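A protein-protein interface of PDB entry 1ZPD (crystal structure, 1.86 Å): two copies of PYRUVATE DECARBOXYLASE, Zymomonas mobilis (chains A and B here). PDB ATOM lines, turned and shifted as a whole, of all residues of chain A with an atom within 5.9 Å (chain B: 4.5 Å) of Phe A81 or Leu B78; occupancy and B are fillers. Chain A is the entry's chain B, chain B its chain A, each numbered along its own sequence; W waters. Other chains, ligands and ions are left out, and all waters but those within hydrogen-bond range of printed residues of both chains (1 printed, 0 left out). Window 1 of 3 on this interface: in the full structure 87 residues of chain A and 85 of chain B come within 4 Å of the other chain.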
ATOM      1  N   GLY A  76       8.948 -12.358  -3.067  1.00  0.00           N
ATOM      2  CA  GLY A  76       8.111 -12.371  -1.854  1.00  0.00           C
ATOM      3  C   GLY A  76       6.660 -12.792  -2.136  1.00  0.00           C
ATOM      4  O   GLY A  76       6.063 -13.597  -1.411  1.00  0.00           O
ATOM      5  N   ALA A  77       6.077 -12.346  -3.250  1.00  0.00           N
ATOM      6  CA  ALA A  77       4.666 -12.657  -3.524  1.00  0.00           C
ATOM      7  C   ALA A  77       4.390 -14.090  -3.896  1.00  0.00           C
ATOM      8  O   ALA A  77       3.373 -14.670  -3.461  1.00  0.00           O
ATOM      9  CB  ALA A  77       4.167 -11.743  -4.655  1.00  0.00           C
ATOM     10  N   LEU A  78       5.273 -14.729  -4.697  1.00  0.00           N
ATOM     11  CA  LEU A  78       4.958 -16.081  -5.166  1.00  0.00           C
ATOM     12  C   LEU A  78       4.810 -17.072  -4.037  1.00  0.00           C
ATOM     13  O   LEU A  78       3.882 -17.903  -4.120  1.00  0.00           O
ATOM     14  CB  LEU A  78       5.975 -16.508  -6.255  1.00  0.00           C
ATOM     15  CG  LEU A  78       5.548 -16.267  -7.708  1.00  0.00           C
ATOM     16  CD1 LEU A  78       5.281 -14.798  -7.973  1.00  0.00           C
ATOM     17  CD2 LEU A  78       6.632 -16.772  -8.685  1.00  0.00           C
ATOM     18  N   SER A  79       5.659 -17.012  -2.996  1.00  0.00           N
ATOM     19  CA  SER A  79       5.467 -17.903  -1.852  1.00  0.00           C
ATOM     20  C   SER A  79       4.247 -17.447  -1.018  1.00  0.00           C
ATOM     21  O   SER A  79       3.487 -18.287  -0.555  1.00  0.00           O
ATOM     22  CB  SER A  79       6.695 -17.974  -0.930  1.00  0.00           C
ATOM     23  OG  SER A  79       7.127 -16.680  -0.593  1.00  0.00           O
ATOM     24  N   ALA A  80       4.042 -16.148  -0.863  1.00  0.00           N
ATOM     25  CA  ALA A  80       2.852 -15.652  -0.149  1.00  0.00           C
ATOM     26  C   ALA A  80       1.548 -16.121  -0.799  1.00  0.00           C
ATOM     27  O   ALA A  80       0.554 -16.358  -0.086  1.00  0.00           O
ATOM     28  CB  ALA A  80       2.883 -14.140  -0.044  1.00  0.00           C
ATOM     29  N   PHE A  81       1.528 -16.315  -2.120  1.00  0.00           N
ATOM     30  CA  PHE A  81       0.341 -16.845  -2.810  1.00  0.00           C
ATOM     31  C   PHE A  81      -0.172 -18.153  -2.255  1.00  0.00           C
ATOM     32  O   PHE A  81      -1.396 -18.398  -2.299  1.00  0.00           O
ATOM     33  CB  PHE A  81       0.623 -17.040  -4.315  1.00  0.00           C
ATOM     34  CG  PHE A  81       0.655 -15.826  -5.183  1.00  0.00           C
ATOM     35  CD1 PHE A  81       0.280 -14.578  -4.713  1.00  0.00           C
ATOM     36  CD2 PHE A  81       1.046 -15.950  -6.522  1.00  0.00           C
ATOM     37  CE1 PHE A  81       0.298 -13.477  -5.541  1.00  0.00           C
ATOM     38  CE2 PHE A  81       1.099 -14.841  -7.343  1.00  0.00           C
ATOM     39  CZ  PHE A  81       0.712 -13.611  -6.860  1.00  0.00           C
ATOM     40  N   ASP A  82       0.687 -19.054  -1.748  1.00  0.00           N
ATOM     41  CA  ASP A  82       0.180 -20.262  -1.110  1.00  0.00           C
ATOM     42  C   ASP A  82      -0.728 -19.931   0.081  1.00  0.00           C
ATOM     43  O   ASP A  82      -1.805 -20.517   0.258  1.00  0.00           O
ATOM     44  CB  ASP A  82       1.374 -21.121  -0.668  1.00  0.00           C
ATOM     45  CG  ASP A  82       1.068 -22.576  -0.473  1.00  0.00           C
ATOM     46  OD1 ASP A  82      -0.113 -22.942  -0.247  1.00  0.00           O
ATOM     47  OD2 ASP A  82       2.041 -23.388  -0.563  1.00  0.00           O
ATOM     48  N   ALA A  83      -0.290 -18.995   0.916  1.00  0.00           N
ATOM     49  CA  ALA A  83      -1.077 -18.555   2.080  1.00  0.00           C
ATOM     50  C   ALA A  83      -2.333 -17.775   1.661  1.00  0.00           C
ATOM     51  O   ALA A  83      -3.374 -17.850   2.343  1.00  0.00           O
ATOM     52  CB  ALA A  83      -0.165 -17.674   2.939  1.00  0.00           C
ATOM     53  N   ILE A  84      -2.247 -17.017   0.576  1.00  0.00           N
ATOM     54  CA  ILE A  84      -3.434 -16.267   0.076  1.00  0.00           C
ATOM     55  C   ILE A  84      -4.467 -17.234  -0.480  1.00  0.00           C
ATOM     56  O   ILE A  84      -5.675 -17.087  -0.192  1.00  0.00           O
ATOM     57  CB  ILE A  84      -2.986 -15.218  -0.941  1.00  0.00           C
ATOM     58  CG1 ILE A  84      -2.185 -14.118  -0.235  1.00  0.00           C
ATOM     59  CG2 ILE A  84      -4.155 -14.633  -1.744  1.00  0.00           C
ATOM     60  CD1 ILE A  84      -2.857 -13.481   0.971  1.00  0.00           C
ATOM     61  N   GLY A  85      -4.029 -18.264  -1.226  1.00  0.00           N
ATOM     62  CA  GLY A  85      -4.969 -19.311  -1.646  1.00  0.00           C
ATOM     63  C   GLY A  85      -5.603 -19.953  -0.413  1.00  0.00           C
ATOM     64  O   GLY A  85      -6.787 -20.327  -0.382  1.00  0.00           O
ATOM     65  N   GLY A  86      -4.812 -20.133   0.649  1.00  0.00           N
ATOM     66  CA  GLY A  86      -5.315 -20.620   1.937  1.00  0.00           C
ATOM     67  C   GLY A  86      -6.408 -19.701   2.500  1.00  0.00           C
ATOM     68  O   GLY A  86      -7.422 -20.223   2.993  1.00  0.00           O
ATOM     69  N   LEU A  96      -3.394  -8.997   0.436  1.00  0.00           N
ATOM     70  CA  LEU A  96      -1.958  -9.095   0.103  1.00  0.00           C
ATOM     71  C   LEU A  96      -1.547  -7.858  -0.683  1.00  0.00           C
ATOM     72  O   LEU A  96      -2.158  -7.609  -1.727  1.00  0.00           O
ATOM     73  CB  LEU A  96      -1.617 -10.325  -0.753  1.00  0.00           C
ATOM     74  CG  LEU A  96      -0.097 -10.445  -1.091  1.00  0.00           C
ATOM     75  CD1 LEU A  96       0.727 -10.698   0.166  1.00  0.00           C
ATOM     76  CD2 LEU A  96       0.104 -11.557  -2.119  1.00  0.00           C
ATOM     77  N   GLN A 124       2.735 -11.723 -12.384  1.00  0.00           N
ATOM     78  CA  GLN A 124       2.343 -11.846 -10.984  1.00  0.00           C
ATOM     79  C   GLN A 124       0.859 -11.486 -10.766  1.00  0.00           C
ATOM     80  O   GLN A 124       0.137 -12.228 -10.106  1.00  0.00           O
ATOM     81  CB  GLN A 124       3.233 -10.958 -10.091  1.00  0.00           C
ATOM     82  CG  GLN A 124       2.920 -11.104  -8.605  1.00  0.00           C
ATOM     83  CD  GLN A 124       3.931 -10.400  -7.720  1.00  0.00           C
ATOM     84  OE1 GLN A 124       5.092 -10.850  -7.631  1.00  0.00           O
ATOM     85  NE2 GLN A 124       3.548  -9.318  -7.037  1.00  0.00           N
ATOM     86  N   LEU A 125       0.423 -10.367 -11.331  1.00  0.00           N
ATOM     87  CA  LEU A 125      -1.008  -9.996 -11.280  1.00  0.00           C
ATOM     88  C   LEU A 125      -1.903 -11.074 -11.879  1.00  0.00           C
ATOM     89  O   LEU A 125      -2.930 -11.452 -11.282  1.00  0.00           O
ATOM     90  CB  LEU A 125      -1.216  -8.677 -12.041  1.00  0.00           C
ATOM     91  CG  LEU A 125      -2.698  -8.302 -12.330  1.00  0.00           C
ATOM     92  CD1 LEU A 125      -3.420  -7.933 -11.030  1.00  0.00           C
ATOM     93  CD2 LEU A 125      -2.756  -7.181 -13.363  1.00  0.00           C
ATOM     94  N   MET A 127      -1.292 -14.295 -12.269  1.00  0.00           N
ATOM     95  CA  MET A 127      -1.288 -15.398 -11.328  1.00  0.00           C
ATOM     96  C   MET A 127      -2.222 -15.140 -10.137  1.00  0.00           C
ATOM     97  O   MET A 127      -3.036 -15.992  -9.776  1.00  0.00           O
ATOM     98  CB  MET A 127       0.156 -15.689 -10.822  1.00  0.00           C
ATOM     99  CG  MET A 127       1.014 -16.355 -11.919  1.00  0.00           C
ATOM    100  SD  MET A 127       2.766 -16.496 -11.432  1.00  0.00           S
ATOM    101  CE  MET A 127       2.712 -17.997 -10.462  1.00  0.00           C
ATOM    102  N   ALA A 128      -2.144 -13.958  -9.532  1.00  0.00           N
ATOM    103  CA  ALA A 128      -2.972 -13.605  -8.365  1.00  0.00           C
ATOM    104  C   ALA A 128      -4.478 -13.662  -8.647  1.00  0.00           C
ATOM    105  O   ALA A 128      -5.275 -14.043  -7.762  1.00  0.00           O
ATOM    106  CB  ALA A 128      -2.596 -12.214  -7.875  1.00  0.00           C
ATOM    107  N   ILE A 131      -6.559 -16.836  -7.471  1.00  0.00           N
ATOM    108  CA  ILE A 131      -6.737 -17.222  -6.078  1.00  0.00           C
ATOM    109  C   ILE A 131      -7.293 -16.106  -5.196  1.00  0.00           C
ATOM    110  O   ILE A 131      -7.138 -16.127  -3.964  1.00  0.00           O
ATOM    111  CB  ILE A 131      -5.369 -17.692  -5.482  1.00  0.00           C
ATOM    112  CG1 ILE A 131      -4.276 -16.641  -5.686  1.00  0.00           C
ATOM    113  CG2 ILE A 131      -4.946 -19.035  -6.089  1.00  0.00           C
ATOM    114  CD1 ILE A 131      -2.946 -16.891  -4.966  1.00  0.00           C
ATOM    115  N   TYR A 163      -5.785  -8.961  -3.770  1.00  0.00           N
ATOM    116  CA  TYR A 163      -4.424  -8.606  -4.165  1.00  0.00           C
ATOM    117  C   TYR A 163      -4.302  -7.167  -4.628  1.00  0.00           C
ATOM    118  O   TYR A 163      -5.073  -6.707  -5.486  1.00  0.00           O
ATOM    119  CB  TYR A 163      -3.973  -9.556  -5.294  1.00  0.00           C
ATOM    120  CG  TYR A 163      -2.661  -9.217  -5.986  1.00  0.00           C
ATOM    121  CD1 TYR A 163      -1.448  -9.735  -5.511  1.00  0.00           C
ATOM    122  CD2 TYR A 163      -2.621  -8.427  -7.123  1.00  0.00           C
ATOM    123  CE1 TYR A 163      -0.236  -9.442  -6.139  1.00  0.00           C
ATOM    124  CE2 TYR A 163      -1.423  -8.134  -7.769  1.00  0.00           C
ATOM    125  CZ  TYR A 163      -0.227  -8.651  -7.268  1.00  0.00           C
ATOM    126  OH  TYR A 163       0.961  -8.356  -7.916  1.00  0.00           O
ATOM    127  N   TRP A 412      -8.052 -25.844   3.224  1.00  0.00           N
ATOM    128  CA  TRP A 412      -6.722 -25.738   2.575  1.00  0.00           C
ATOM    129  C   TRP A 412      -5.790 -26.847   3.088  1.00  0.00           C
ATOM    130  O   TRP A 412      -5.171 -27.555   2.287  1.00  0.00           O
ATOM    131  CB  TRP A 412      -6.078 -24.399   2.851  1.00  0.00           C
ATOM    132  CG  TRP A 412      -4.999 -23.914   1.922  1.00  0.00           C
ATOM    133  CD1 TRP A 412      -3.726 -23.541   2.284  1.00  0.00           C
ATOM    134  CD2 TRP A 412      -5.092 -23.697   0.505  1.00  0.00           C
ATOM    135  NE1 TRP A 412      -3.018 -23.120   1.170  1.00  0.00           N
ATOM    136  CE2 TRP A 412      -3.838 -23.215   0.066  1.00  0.00           C
ATOM    137  CE3 TRP A 412      -6.129 -23.875  -0.441  1.00  0.00           C
ATOM    138  CZ2 TRP A 412      -3.581 -22.899  -1.272  1.00  0.00           C
ATOM    139  CZ3 TRP A 412      -5.862 -23.565  -1.770  1.00  0.00           C
ATOM    140  CH2 TRP A 412      -4.600 -23.078  -2.179  1.00  0.00           C
ATOM    141  N   SER B  74      -1.426 -27.934  -5.044  1.00  0.00           N
ATOM    142  CA  SER B  74      -1.855 -26.660  -4.487  1.00  0.00           C
ATOM    143  C   SER B  74      -1.106 -26.181  -3.252  1.00  0.00           C
ATOM    144  O   SER B  74      -0.279 -25.264  -3.363  1.00  0.00           O
ATOM    145  CB  SER B  74      -3.396 -26.675  -4.258  1.00  0.00           C
ATOM    146  OG  SER B  74      -3.838 -25.339  -4.069  1.00  0.00           O
ATOM    147  N   GLY B  76       1.345 -27.687  -1.854  1.00  0.00           N
ATOM    148  CA  GLY B  76       2.774 -27.957  -2.117  1.00  0.00           C
ATOM    149  C   GLY B  76       3.308 -27.187  -3.310  1.00  0.00           C
ATOM    150  O   GLY B  76       4.355 -26.531  -3.259  1.00  0.00           O
ATOM    151  N   ALA B  77       2.537 -27.139  -4.405  1.00  0.00           N
ATOM    152  CA  ALA B  77       2.998 -26.512  -5.640  1.00  0.00           C
ATOM    153  C   ALA B  77       3.056 -25.000  -5.578  1.00  0.00           C
ATOM    154  O   ALA B  77       4.009 -24.413  -6.113  1.00  0.00           O
ATOM    155  CB  ALA B  77       2.108 -26.976  -6.810  1.00  0.00           C
ATOM    156  N   LEU B  78       2.100 -24.325  -4.912  1.00  0.00           N
ATOM    157  CA  LEU B  78       2.102 -22.870  -4.957  1.00  0.00           C
ATOM    158  C   LEU B  78       3.355 -22.263  -4.314  1.00  0.00           C
ATOM    159  O   LEU B  78       3.908 -21.329  -4.908  1.00  0.00           O
ATOM    160  CB  LEU B  78       0.791 -22.312  -4.348  1.00  0.00           C
ATOM    161  CG  LEU B  78      -0.336 -22.024  -5.361  1.00  0.00           C
ATOM    162  CD1 LEU B  78      -0.732 -23.258  -6.159  1.00  0.00           C
ATOM    163  CD2 LEU B  78      -1.593 -21.466  -4.653  1.00  0.00           C
ATOM    164  N   SER B  79       3.855 -22.803  -3.197  1.00  0.00           N
ATOM    165  CA  SER B  79       5.109 -22.293  -2.631  1.00  0.00           C
ATOM    166  C   SER B  79       6.307 -22.690  -3.517  1.00  0.00           C
ATOM    167  O   SER B  79       7.196 -21.877  -3.760  1.00  0.00           O
ATOM    168  CB  SER B  79       5.340 -22.738  -1.181  1.00  0.00           C
ATOM    169  OG  SER B  79       5.137 -24.129  -1.060  1.00  0.00           O
ATOM    170  N   ALA B  80       6.306 -23.912  -4.037  1.00  0.00           N
ATOM    171  CA  ALA B  80       7.374 -24.383  -4.935  1.00  0.00           C
ATOM    172  C   ALA B  80       7.465 -23.529  -6.193  1.00  0.00           C
ATOM    173  O   ALA B  80       8.581 -23.312  -6.709  1.00  0.00           O
ATOM    174  CB  ALA B  80       7.111 -25.839  -5.315  1.00  0.00           C
ATOM    175  N   PHE B  81       6.357 -22.927  -6.659  1.00  0.00           N
ATOM    176  CA  PHE B  81       6.406 -21.965  -7.748  1.00  0.00           C
ATOM    177  C   PHE B  81       7.414 -20.854  -7.551  1.00  0.00           C
ATOM    178  O   PHE B  81       8.003 -20.409  -8.547  1.00  0.00           O
ATOM    179  CB  PHE B  81       5.003 -21.393  -8.026  1.00  0.00           C
ATOM    180  CG  PHE B  81       4.003 -22.269  -8.728  1.00  0.00           C
ATOM    181  CD1 PHE B  81       4.344 -23.487  -9.296  1.00  0.00           C
ATOM    182  CD2 PHE B  81       2.676 -21.835  -8.862  1.00  0.00           C
ATOM    183  CE1 PHE B  81       3.412 -24.267  -9.959  1.00  0.00           C
ATOM    184  CE2 PHE B  81       1.731 -22.613  -9.518  1.00  0.00           C
ATOM    185  CZ  PHE B  81       2.087 -23.832 -10.063  1.00  0.00           C
ATOM    186  N   ASP B  82       7.656 -20.346  -6.333  1.00  0.00           N
ATOM    187  CA  ASP B  82       8.656 -19.300  -6.138  1.00  0.00           C
ATOM    188  C   ASP B  82      10.061 -19.801  -6.546  1.00  0.00           C
ATOM    189  O   ASP B  82      10.812 -19.142  -7.279  1.00  0.00           O
ATOM    190  CB  ASP B  82       8.647 -18.848  -4.673  1.00  0.00           C
ATOM    191  CG  ASP B  82       9.265 -17.512  -4.399  1.00  0.00           C
ATOM    192  OD1 ASP B  82      10.092 -17.009  -5.193  1.00  0.00           O
ATOM    193  OD2 ASP B  82       8.910 -16.925  -3.333  1.00  0.00           O
ATOM    194  N   GLN B 124      -4.052 -24.270 -11.039  1.00  0.00           N
ATOM    195  CA  GLN B 124      -2.606 -24.511 -10.803  1.00  0.00           C
ATOM    196  C   GLN B 124      -1.836 -24.602 -12.129  1.00  0.00           C
ATOM    197  O   GLN B 124      -0.777 -23.979 -12.279  1.00  0.00           O
ATOM    198  CB  GLN B 124      -2.418 -25.794  -9.994  1.00  0.00           C
ATOM    199  CG  GLN B 124      -0.952 -26.032  -9.599  1.00  0.00           C
ATOM    200  CD  GLN B 124      -0.801 -27.166  -8.615  1.00  0.00           C
ATOM    201  OE1 GLN B 124      -1.183 -27.037  -7.440  1.00  0.00           O
ATOM    202  NE2 GLN B 124      -0.237 -28.298  -9.048  1.00  0.00           N
ATOM    203  N   MET B 127      -1.561 -21.152 -13.658  1.00  0.00           N
ATOM    204  CA  MET B 127      -0.540 -20.380 -12.960  1.00  0.00           C
ATOM    205  C   MET B 127       0.871 -20.836 -13.380  1.00  0.00           C
ATOM    206  O   MET B 127       1.718 -20.011 -13.695  1.00  0.00           O
ATOM    207  CB  MET B 127      -0.722 -20.531 -11.430  1.00  0.00           C
ATOM    208  CG  MET B 127      -1.920 -19.747 -10.870  1.00  0.00           C
ATOM    209  SD  MET B 127      -2.291 -20.118  -9.130  1.00  0.00           S
ATOM    210  CE  MET B 127      -1.135 -18.999  -8.326  1.00  0.00           C
HETATM  211  O   HOH W   1       2.760 -19.204  -6.299  1.00  0.00           O
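Of the 10 printed residues of chain B, 6 touch a printed residue of chain A. Printed residues of chain B that touch a printed residue of chain A: Ser B74, Leu B78, Ser B79, Phe B81, Asp B82 and Met B127. Hydrophobic or aromatic side chains of chain B that line the printed part of chain A: Leu B78 and Met B127. Among the printed residues, no Asp or Glu carboxylate lies within 4 Å of a Lys or Arg side-chain nitrogen of the other chain.
Of chain B, only Leu B78 comes within 4 Å of Phe A81. Leu B78 touches just these residues of chain A: Leu A78, Phe A81 and Asp A82. Of the printed residues of chain B, Asp A82 touches Ser B74, Leu B78 and Ser B79. Of the printed residues of chain A, Phe B81 touches Leu A78 (3.9 Å). Of the printed residues of chain A, Ser B79 touches Asp A82 (3.2 Å). Of the printed residues of chain B, Trp A412 touches Ser B74. Printed residues of chain A within 4 Å of Ser B74: Asp A82 and Trp A412. Gly A85 touches none of the printed residues of chain B. The nearest residue of chain B that does not touch Phe A81 is Met B127 (4.2 Å). The nearest printed residue of chain B that does not touch Leu A78 is Ser B79 (4.8 Å).
Leu A78 touches its own counterpart, Leu B78. Leu A78 touches Phe B81, and with the chains exchanged Phe A81 touches Leu B78. Leu A78 touches Asp B82, and with the chains exchanged Asp A82 touches Leu B78. Met A127 touches its own counterpart, Met B127. Positions printed for both chains: 76, 77, 78, 79, 80, 81, 82, 124 and 127.
The backbone carbonyl oxygen of Gly B76 is in hydrogen-bond range of the side-chain hydroxyl of Ser B79, 3.3 Å away. The backbone carbonyl oxygen (O) of Gly A76 sits at hydrogen-bond distance from the side-chain hydroxyl (OG) of Ser A79 (3.4 Å). OE1 of Gln B124 lies within hydrogen-bond range of N of Ser B74 (2.6 Å). The backbone carbonyl oxygen of Asp A82 is in hydrogen-bond range of the indole nitrogen of Trp A412, at 3.0 Å.
OD2 of Asp B82 lies within hydrogen-bond range of N of Ser A79, 3.3 Å away. The side-chain hydroxyl (OG) of Ser B79 sits at hydrogen-bond distance from the side-chain carboxylate (OD2) of Asp A82.
Leu A78 touches Leu B78 (O to O, 3.5 Å). Phe B81 touches Leu A78 (O to CD2, 3.9 Å). Asp B82 touches Leu A78. CD2 of Leu B78 touches O of Phe A81 (3.9 Å). O of Ser B74 touches OD1 of Asp A82 (3.9 Å). Leu B78 touches Asp A82. Met A127 touches Met B127 (O to CE, 3.8 Å). CH2 of Trp A412 touches OG of Ser B74 (3.0 Å).
Water W1 lies within hydrogen-bond range of O of Leu A78 (2.8 Å) and O of Leu B78 (2.8 Å).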
